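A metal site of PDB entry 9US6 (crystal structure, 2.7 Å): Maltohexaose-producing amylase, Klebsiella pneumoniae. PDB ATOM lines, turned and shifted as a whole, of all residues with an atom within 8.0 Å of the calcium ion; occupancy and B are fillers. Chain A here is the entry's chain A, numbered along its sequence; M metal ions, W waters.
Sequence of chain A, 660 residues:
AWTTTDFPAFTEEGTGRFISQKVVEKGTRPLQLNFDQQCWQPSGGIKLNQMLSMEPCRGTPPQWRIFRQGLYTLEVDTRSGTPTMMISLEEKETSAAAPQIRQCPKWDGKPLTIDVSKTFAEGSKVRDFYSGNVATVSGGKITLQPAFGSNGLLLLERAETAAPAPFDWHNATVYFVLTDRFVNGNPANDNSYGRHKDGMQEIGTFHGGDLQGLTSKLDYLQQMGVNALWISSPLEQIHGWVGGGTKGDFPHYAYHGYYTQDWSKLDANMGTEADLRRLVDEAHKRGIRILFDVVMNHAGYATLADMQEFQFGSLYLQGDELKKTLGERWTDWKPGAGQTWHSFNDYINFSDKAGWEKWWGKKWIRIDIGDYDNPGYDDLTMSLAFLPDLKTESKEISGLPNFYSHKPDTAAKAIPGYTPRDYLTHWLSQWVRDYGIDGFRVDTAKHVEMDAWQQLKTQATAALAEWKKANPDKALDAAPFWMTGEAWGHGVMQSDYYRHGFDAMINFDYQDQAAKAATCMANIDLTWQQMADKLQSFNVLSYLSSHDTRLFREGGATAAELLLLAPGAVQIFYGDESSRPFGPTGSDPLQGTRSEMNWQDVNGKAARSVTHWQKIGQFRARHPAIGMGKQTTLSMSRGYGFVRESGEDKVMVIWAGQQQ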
ATOM      1  N   MET A 296     -23.348 -24.526   1.459  1.00  0.00           N
ATOM      2  CA  MET A 296     -23.975 -23.849   2.578  1.00  0.00           C
ATOM      3  C   MET A 296     -23.051 -23.804   3.806  1.00  0.00           C
ATOM      4  O   MET A 296     -23.388 -23.149   4.788  1.00  0.00           O
ATOM      5  CB  MET A 296     -25.312 -24.500   2.960  1.00  0.00           C
ATOM      6  CG  MET A 296     -26.489 -24.015   2.122  1.00  0.00           C
ATOM      7  SD  MET A 296     -28.036 -24.889   2.431  1.00  0.00           S
ATOM      8  CE  MET A 296     -28.246 -24.604   4.197  1.00  0.00           C
ATOM      9  N   ASN A 297     -21.897 -24.474   3.757  1.00  0.00           N
ATOM     10  CA  ASN A 297     -21.015 -24.545   4.918  1.00  0.00           C
ATOM     11  C   ASN A 297     -20.346 -23.192   5.167  1.00  0.00           C
ATOM     12  O   ASN A 297     -20.259 -22.736   6.303  1.00  0.00           O
ATOM     13  CB  ASN A 297     -19.946 -25.610   4.764  1.00  0.00           C
ATOM     14  CG  ASN A 297     -19.086 -25.742   6.001  1.00  0.00           C
ATOM     15  OD1 ASN A 297     -19.586 -26.114   7.061  1.00  0.00           O
ATOM     16  ND2 ASN A 297     -17.796 -25.457   5.883  1.00  0.00           N
ATOM     17  N   HIS A 298     -19.887 -22.557   4.080  1.00  0.00           N
ATOM     18  CA  HIS A 298     -18.968 -21.445   4.194  1.00  0.00           C
ATOM     19  C   HIS A 298     -19.211 -20.427   3.082  1.00  0.00           C
ATOM     20  O   HIS A 298     -19.725 -20.761   2.026  1.00  0.00           O
ATOM     21  CB  HIS A 298     -17.523 -21.953   4.139  1.00  0.00           C
ATOM     22  CG  HIS A 298     -17.217 -22.778   2.927  1.00  0.00           C
ATOM     23  ND1 HIS A 298     -17.233 -24.163   2.939  1.00  0.00           N
ATOM     24  CD2 HIS A 298     -16.896 -22.424   1.671  1.00  0.00           C
ATOM     25  CE1 HIS A 298     -16.928 -24.612   1.724  1.00  0.00           C
ATOM     26  NE2 HIS A 298     -16.728 -23.575   0.940  1.00  0.00           N
ATOM     27  N   ARG A 366     -18.951 -18.045  11.784  1.00  0.00           N
ATOM     28  CA  ARG A 366     -17.907 -18.295  12.765  1.00  0.00           C
ATOM     29  C   ARG A 366     -16.543 -18.165  12.086  1.00  0.00           C
ATOM     30  O   ARG A 366     -16.349 -18.702  10.995  1.00  0.00           O
ATOM     31  CB  ARG A 366     -18.005 -19.710  13.357  1.00  0.00           C
ATOM     32  CG  ARG A 366     -18.972 -19.903  14.514  1.00  0.00           C
ATOM     33  CD  ARG A 366     -19.123 -21.377  14.856  1.00  0.00           C
ATOM     34  NE  ARG A 366     -19.729 -22.111  13.743  1.00  0.00           N
ATOM     35  CZ  ARG A 366     -21.021 -22.393  13.586  1.00  0.00           C
ATOM     36  NH1 ARG A 366     -21.430 -23.027  12.509  1.00  0.00           N
ATOM     37  NH2 ARG A 366     -21.908 -22.019  14.496  1.00  0.00           N
ATOM     38  N   ASP A 378     -15.176 -29.270  16.166  1.00  0.00           N
ATOM     39  CA  ASP A 378     -15.813 -30.431  15.567  1.00  0.00           C
ATOM     40  C   ASP A 378     -16.126 -30.106  14.107  1.00  0.00           C
ATOM     41  O   ASP A 378     -16.007 -28.963  13.680  1.00  0.00           O
ATOM     42  CB  ASP A 378     -17.043 -30.833  16.353  1.00  0.00           C
ATOM     43  CG  ASP A 378     -18.101 -29.753  16.495  1.00  0.00           C
ATOM     44  OD1 ASP A 378     -18.854 -29.537  15.527  1.00  0.00           O
ATOM     45  OD2 ASP A 378     -18.122 -29.092  17.558  1.00  0.00           O
ATOM     46  N   ASP A 379     -16.555 -31.131  13.359  1.00  0.00           N
ATOM     47  CA  ASP A 379     -16.830 -30.997  11.936  1.00  0.00           C
ATOM     48  C   ASP A 379     -17.817 -29.850  11.665  1.00  0.00           C
ATOM     49  O   ASP A 379     -17.632 -29.112  10.690  1.00  0.00           O
ATOM     50  CB  ASP A 379     -17.325 -32.312  11.349  1.00  0.00           C
ATOM     51  CG  ASP A 379     -16.269 -33.416  11.234  1.00  0.00           C
ATOM     52  OD1 ASP A 379     -15.201 -33.155  10.646  1.00  0.00           O
ATOM     53  OD2 ASP A 379     -16.538 -34.532  11.724  1.00  0.00           O
ATOM     54  N   LEU A 380     -18.839 -29.695  12.520  1.00  0.00           N
ATOM     55  CA  LEU A 380     -20.006 -28.876  12.193  1.00  0.00           C
ATOM     56  C   LEU A 380     -19.720 -27.394  12.422  1.00  0.00           C
ATOM     57  O   LEU A 380     -20.253 -26.563  11.688  1.00  0.00           O
ATOM     58  CB  LEU A 380     -21.213 -29.329  12.997  1.00  0.00           C
ATOM     59  CG  LEU A 380     -21.705 -30.759  12.746  1.00  0.00           C
ATOM     60  CD1 LEU A 380     -23.063 -30.935  13.401  1.00  0.00           C
ATOM     61  CD2 LEU A 380     -21.757 -31.126  11.268  1.00  0.00           C
ATOM     62  N   THR A 381     -18.919 -27.065  13.427  1.00  0.00           N
ATOM     63  CA  THR A 381     -18.749 -25.681  13.819  1.00  0.00           C
ATOM     64  C   THR A 381     -17.328 -25.192  13.547  1.00  0.00           C
ATOM     65  O   THR A 381     -17.038 -24.011  13.772  1.00  0.00           O
ATOM     66  CB  THR A 381     -19.126 -25.532  15.295  1.00  0.00           C
ATOM     67  OG1 THR A 381     -18.400 -26.537  15.986  1.00  0.00           O
ATOM     68  CG2 THR A 381     -20.612 -25.724  15.527  1.00  0.00           C
ATOM     69  N   MET A 382     -16.440 -26.057  13.035  1.00  0.00           N
ATOM     70  CA  MET A 382     -15.075 -25.650  12.746  1.00  0.00           C
ATOM     71  C   MET A 382     -15.049 -24.747  11.518  1.00  0.00           C
ATOM     72  O   MET A 382     -15.974 -24.769  10.701  1.00  0.00           O
ATOM     73  CB  MET A 382     -14.147 -26.848  12.487  1.00  0.00           C
ATOM     74  CG  MET A 382     -14.527 -27.697  11.276  1.00  0.00           C
ATOM     75  SD  MET A 382     -13.334 -29.005  10.938  1.00  0.00           S
ATOM     76  CE  MET A 382     -12.359 -28.211   9.657  1.00  0.00           C
ATOM     77  N   SER A 383     -13.971 -23.955  11.423  1.00  0.00           N
ATOM     78  CA  SER A 383     -13.677 -23.148  10.254  1.00  0.00           C
ATOM     79  C   SER A 383     -12.797 -23.953   9.299  1.00  0.00           C
ATOM     80  O   SER A 383     -11.603 -24.071   9.517  1.00  0.00           O
ATOM     81  CB  SER A 383     -13.005 -21.848  10.665  1.00  0.00           C
ATOM     82  OG  SER A 383     -12.683 -21.032   9.554  1.00  0.00           O
ATOM     83  N   LEU A 384     -13.424 -24.517   8.266  1.00  0.00           N
ATOM     84  CA  LEU A 384     -12.738 -25.386   7.311  1.00  0.00           C
ATOM     85  C   LEU A 384     -11.737 -24.561   6.499  1.00  0.00           C
ATOM     86  O   LEU A 384     -12.142 -23.714   5.708  1.00  0.00           O
ATOM     87  CB  LEU A 384     -13.780 -26.051   6.409  1.00  0.00           C
ATOM     88  CG  LEU A 384     -13.230 -26.977   5.314  1.00  0.00           C
ATOM     89  CD1 LEU A 384     -12.535 -28.199   5.901  1.00  0.00           C
ATOM     90  CD2 LEU A 384     -14.331 -27.398   4.370  1.00  0.00           C
ATOM     91  N   LEU A 387     -12.084 -20.801   6.407  1.00  0.00           N
ATOM     92  CA  LEU A 387     -13.207 -20.233   5.690  1.00  0.00           C
ATOM     93  C   LEU A 387     -14.273 -19.790   6.686  1.00  0.00           C
ATOM     94  O   LEU A 387     -14.542 -20.496   7.647  1.00  0.00           O
ATOM     95  CB  LEU A 387     -13.785 -21.235   4.695  1.00  0.00           C
ATOM     96  CG  LEU A 387     -13.016 -21.414   3.391  1.00  0.00           C
ATOM     97  CD1 LEU A 387     -13.365 -22.735   2.730  1.00  0.00           C
ATOM     98  CD2 LEU A 387     -13.281 -20.258   2.439  1.00  0.00           C
ATOM     99  N   PRO A 388     -14.938 -18.626   6.499  1.00  0.00           N
ATOM    100  CA  PRO A 388     -16.003 -18.233   7.415  1.00  0.00           C
ATOM    101  C   PRO A 388     -17.110 -19.288   7.443  1.00  0.00           C
ATOM    102  O   PRO A 388     -17.688 -19.603   6.408  1.00  0.00           O
ATOM    103  CB  PRO A 388     -16.455 -16.876   6.883  1.00  0.00           C
ATOM    104  CG  PRO A 388     -16.000 -16.873   5.430  1.00  0.00           C
ATOM    105  CD  PRO A 388     -14.729 -17.671   5.401  1.00  0.00           C
ATOM    106  N   ASP A 389     -17.369 -19.854   8.630  1.00  0.00           N
ATOM    107  CA  ASP A 389     -18.325 -20.934   8.771  1.00  0.00           C
ATOM    108  C   ASP A 389     -19.715 -20.341   9.019  1.00  0.00           C
ATOM    109  O   ASP A 389     -19.961 -19.762  10.065  1.00  0.00           O
ATOM    110  CB  ASP A 389     -17.927 -21.886   9.885  1.00  0.00           C
ATOM    111  CG  ASP A 389     -18.600 -23.246   9.853  1.00  0.00           C
ATOM    112  OD1 ASP A 389     -18.443 -23.950   8.828  1.00  0.00           O
ATOM    113  OD2 ASP A 389     -19.269 -23.603  10.836  1.00  0.00           O
ATOM    114  N   LEU A 390     -20.610 -20.512   8.041  1.00  0.00           N
ATOM    115  CA  LEU A 390     -21.986 -20.044   8.159  1.00  0.00           C
ATOM    116  C   LEU A 390     -22.672 -20.794   9.307  1.00  0.00           C
ATOM    117  O   LEU A 390     -22.477 -21.996   9.464  1.00  0.00           O
ATOM    118  CB  LEU A 390     -22.707 -20.267   6.835  1.00  0.00           C
ATOM    119  CG  LEU A 390     -22.289 -19.355   5.675  1.00  0.00           C
ATOM    120  CD1 LEU A 390     -22.596 -19.975   4.327  1.00  0.00           C
ATOM    121  CD2 LEU A 390     -22.978 -17.995   5.780  1.00  0.00           C
ATOM    122  N   LYS A 391     -23.461 -20.053  10.102  1.00  0.00           N
ATOM    123  CA  LYS A 391     -24.142 -20.587  11.273  1.00  0.00           C
ATOM    124  C   LYS A 391     -25.497 -21.164  10.864  1.00  0.00           C
ATOM    125  O   LYS A 391     -26.533 -20.561  11.108  1.00  0.00           O
ATOM    126  CB  LYS A 391     -24.279 -19.486  12.322  1.00  0.00           C
ATOM    127  CG  LYS A 391     -22.963 -18.929  12.863  1.00  0.00           C
ATOM    128  CD  LYS A 391     -23.053 -17.601  13.590  1.00  0.00           C
ATOM    129  CE  LYS A 391     -23.997 -17.625  14.750  1.00  0.00           C
ATOM    130  NZ  LYS A 391     -23.812 -16.470  15.635  1.00  0.00           N
ATOM    131  N   THR A 392     -25.464 -22.351  10.239  1.00  0.00           N
ATOM    132  CA  THR A 392     -26.653 -22.989   9.687  1.00  0.00           C
ATOM    133  C   THR A 392     -27.584 -23.457  10.806  1.00  0.00           C
ATOM    134  O   THR A 392     -28.777 -23.584  10.599  1.00  0.00           O
ATOM    135  CB  THR A 392     -26.232 -24.151   8.797  1.00  0.00           C
ATOM    136  OG1 THR A 392     -25.259 -24.898   9.515  1.00  0.00           O
ATOM    137  CG2 THR A 392     -25.617 -23.700   7.472  1.00  0.00           C
ATOM    138  N   GLU A 393     -27.009 -23.740  11.978  1.00  0.00           N
ATOM    139  CA  GLU A 393     -27.757 -24.296  13.096  1.00  0.00           C
ATOM    140  C   GLU A 393     -28.375 -23.185  13.956  1.00  0.00           C
ATOM    141  O   GLU A 393     -29.163 -23.475  14.847  1.00  0.00           O
ATOM    142  CB  GLU A 393     -26.867 -25.220  13.939  1.00  0.00           C
ATOM    143  CG  GLU A 393     -25.838 -24.506  14.815  1.00  0.00           C
ATOM    144  CD  GLU A 393     -24.821 -23.629  14.101  1.00  0.00           C
ATOM    145  OE1 GLU A 393     -24.242 -24.078  13.082  1.00  0.00           O
ATOM    146  OE2 GLU A 393     -24.604 -22.487  14.573  1.00  0.00           O
ATOM    147  N   THR A 444     -19.082 -30.173   1.081  1.00  0.00           N
ATOM    148  CA  THR A 444     -18.776 -30.109   2.507  1.00  0.00           C
ATOM    149  C   THR A 444     -19.975 -30.582   3.334  1.00  0.00           C
ATOM    150  O   THR A 444     -20.390 -29.915   4.283  1.00  0.00           O
ATOM    151  CB  THR A 444     -18.328 -28.686   2.859  1.00  0.00           C
ATOM    152  OG1 THR A 444     -19.060 -27.743   2.084  1.00  0.00           O
ATOM    153  CG2 THR A 444     -16.862 -28.474   2.569  1.00  0.00           C
ATOM    154  N   LYS A 446     -20.397 -32.962   5.470  1.00  0.00           N
ATOM    155  CA  LYS A 446     -20.197 -33.445   6.829  1.00  0.00           C
ATOM    156  C   LYS A 446     -19.873 -32.289   7.767  1.00  0.00           C
ATOM    157  O   LYS A 446     -19.652 -32.532   8.963  1.00  0.00           O
ATOM    158  CB  LYS A 446     -19.142 -34.556   6.870  1.00  0.00           C
ATOM    159  CG  LYS A 446     -17.694 -34.164   7.102  1.00  0.00           C
ATOM    160  CD  LYS A 446     -16.725 -35.315   6.832  1.00  0.00           C
ATOM    161  CE  LYS A 446     -15.445 -35.233   7.623  1.00  0.00           C
ATOM    162  NZ  LYS A 446     -15.612 -35.799   8.971  1.00  0.00           N
ATOM    163  N   HIS A 447     -19.873 -31.044   7.272  1.00  0.00           N
ATOM    164  CA  HIS A 447     -19.556 -29.887   8.086  1.00  0.00           C
ATOM    165  C   HIS A 447     -20.789 -29.022   8.338  1.00  0.00           C
ATOM    166  O   HIS A 447     -20.674 -27.938   8.904  1.00  0.00           O
ATOM    167  CB  HIS A 447     -18.446 -29.054   7.429  1.00  0.00           C
ATOM    168  CG  HIS A 447     -17.172 -29.803   7.244  1.00  0.00           C
ATOM    169  ND1 HIS A 447     -16.337 -30.083   8.304  1.00  0.00           N
ATOM    170  CD2 HIS A 447     -16.613 -30.339   6.163  1.00  0.00           C
ATOM    171  CE1 HIS A 447     -15.294 -30.760   7.856  1.00  0.00           C
ATOM    172  NE2 HIS A 447     -15.442 -30.934   6.562  1.00  0.00           N
ATOM    173  N   VAL A 448     -21.961 -29.502   7.888  1.00  0.00           N
ATOM    174  CA  VAL A 448     -23.248 -28.857   8.138  1.00  0.00           C
ATOM    175  C   VAL A 448     -24.185 -29.927   8.694  1.00  0.00           C
ATOM    176  O   VAL A 448     -24.110 -31.086   8.305  1.00  0.00           O
ATOM    177  CB  VAL A 448     -23.829 -28.211   6.856  1.00  0.00           C
ATOM    178  CG1 VAL A 448     -25.225 -27.630   7.070  1.00  0.00           C
ATOM    179  CG2 VAL A 448     -22.911 -27.136   6.289  1.00  0.00           C
ATOM    180  N   GLU A 449     -25.066 -29.517   9.611  1.00  0.00           N
ATOM    181  CA  GLU A 449     -25.953 -30.458  10.281  1.00  0.00           C
ATOM    182  C   GLU A 449     -26.973 -31.013   9.280  1.00  0.00           C
ATOM    183  O   GLU A 449     -27.337 -30.341   8.316  1.00  0.00           O
ATOM    184  CB  GLU A 449     -26.613 -29.823  11.512  1.00  0.00           C
ATOM    185  CG  GLU A 449     -27.592 -28.688  11.211  1.00  0.00           C
ATOM    186  CD  GLU A 449     -26.991 -27.310  10.962  1.00  0.00           C
ATOM    187  OE1 GLU A 449     -25.760 -27.137  11.041  1.00  0.00           O
ATOM    188  OE2 GLU A 449     -27.796 -26.400  10.683  1.00  0.00           O
HETATM  189 CA    CA M   1     -19.989 -25.700   9.593  1.00  0.00          CA
HETATM  190  O   HOH W   1     -17.713 -26.544   9.908  1.00  0.00           O
HETATM  191  O   HOH W   2     -21.078 -24.137   8.407  1.00  0.00           O
HETATM  192  O   HOH W   3     -22.268 -25.510  10.393  1.00  0.00           O
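The backbone NH of Leu 380 lies within hydrogen-bond range of the side-chain carboxylate of Asp 378, 3.0 Å away. ND1 of His 447 sits at hydrogen-bond distance from O of Asp 379 (2.9 Å). The backbone carbonyl oxygen (O) of Asp 389 is in hydrogen-bond range of the backbone NH (N) of Arg 366. N of Leu 390 lies within hydrogen-bond range of O of Asn 297, 2.8 Å away. A ring nitrogen (ND1) of His 298 sits at hydrogen-bond distance from the side-chain amide nitrogen (ND2) of Asn 297 (3.3 Å).
Within 4 Å of the calcium ion: Asn 297, Leu 380, Asp 389 and His 447.
Water W2 binds the calcium ion, 2.2 Å away. O of Leu 380 is bound to the calcium ion, 2.3 Å away. Water W3 binds the calcium ion, at 2.4 Å. The calcium ion is bound by the backbone carbonyl oxygen (O) of His 447 (2.4 Å). Water W1 binds the calcium ion (2.4 Å). The calcium ion is bound by OD1 of Asp 389. OD2 of Asp 389 is bound to the calcium ion (2.5 Å). OD1 of Asn 297 is bound to the calcium ion (2.6 Å). The calcium ion has eight donor atoms within binding distance.
Water W2 bridges O of Asn 297 (2.7 Å) and O of Leu 390 (2.8 Å). Water W3 lies within hydrogen-bond range of OG1 of Thr 392 and NH1 of Arg 366.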
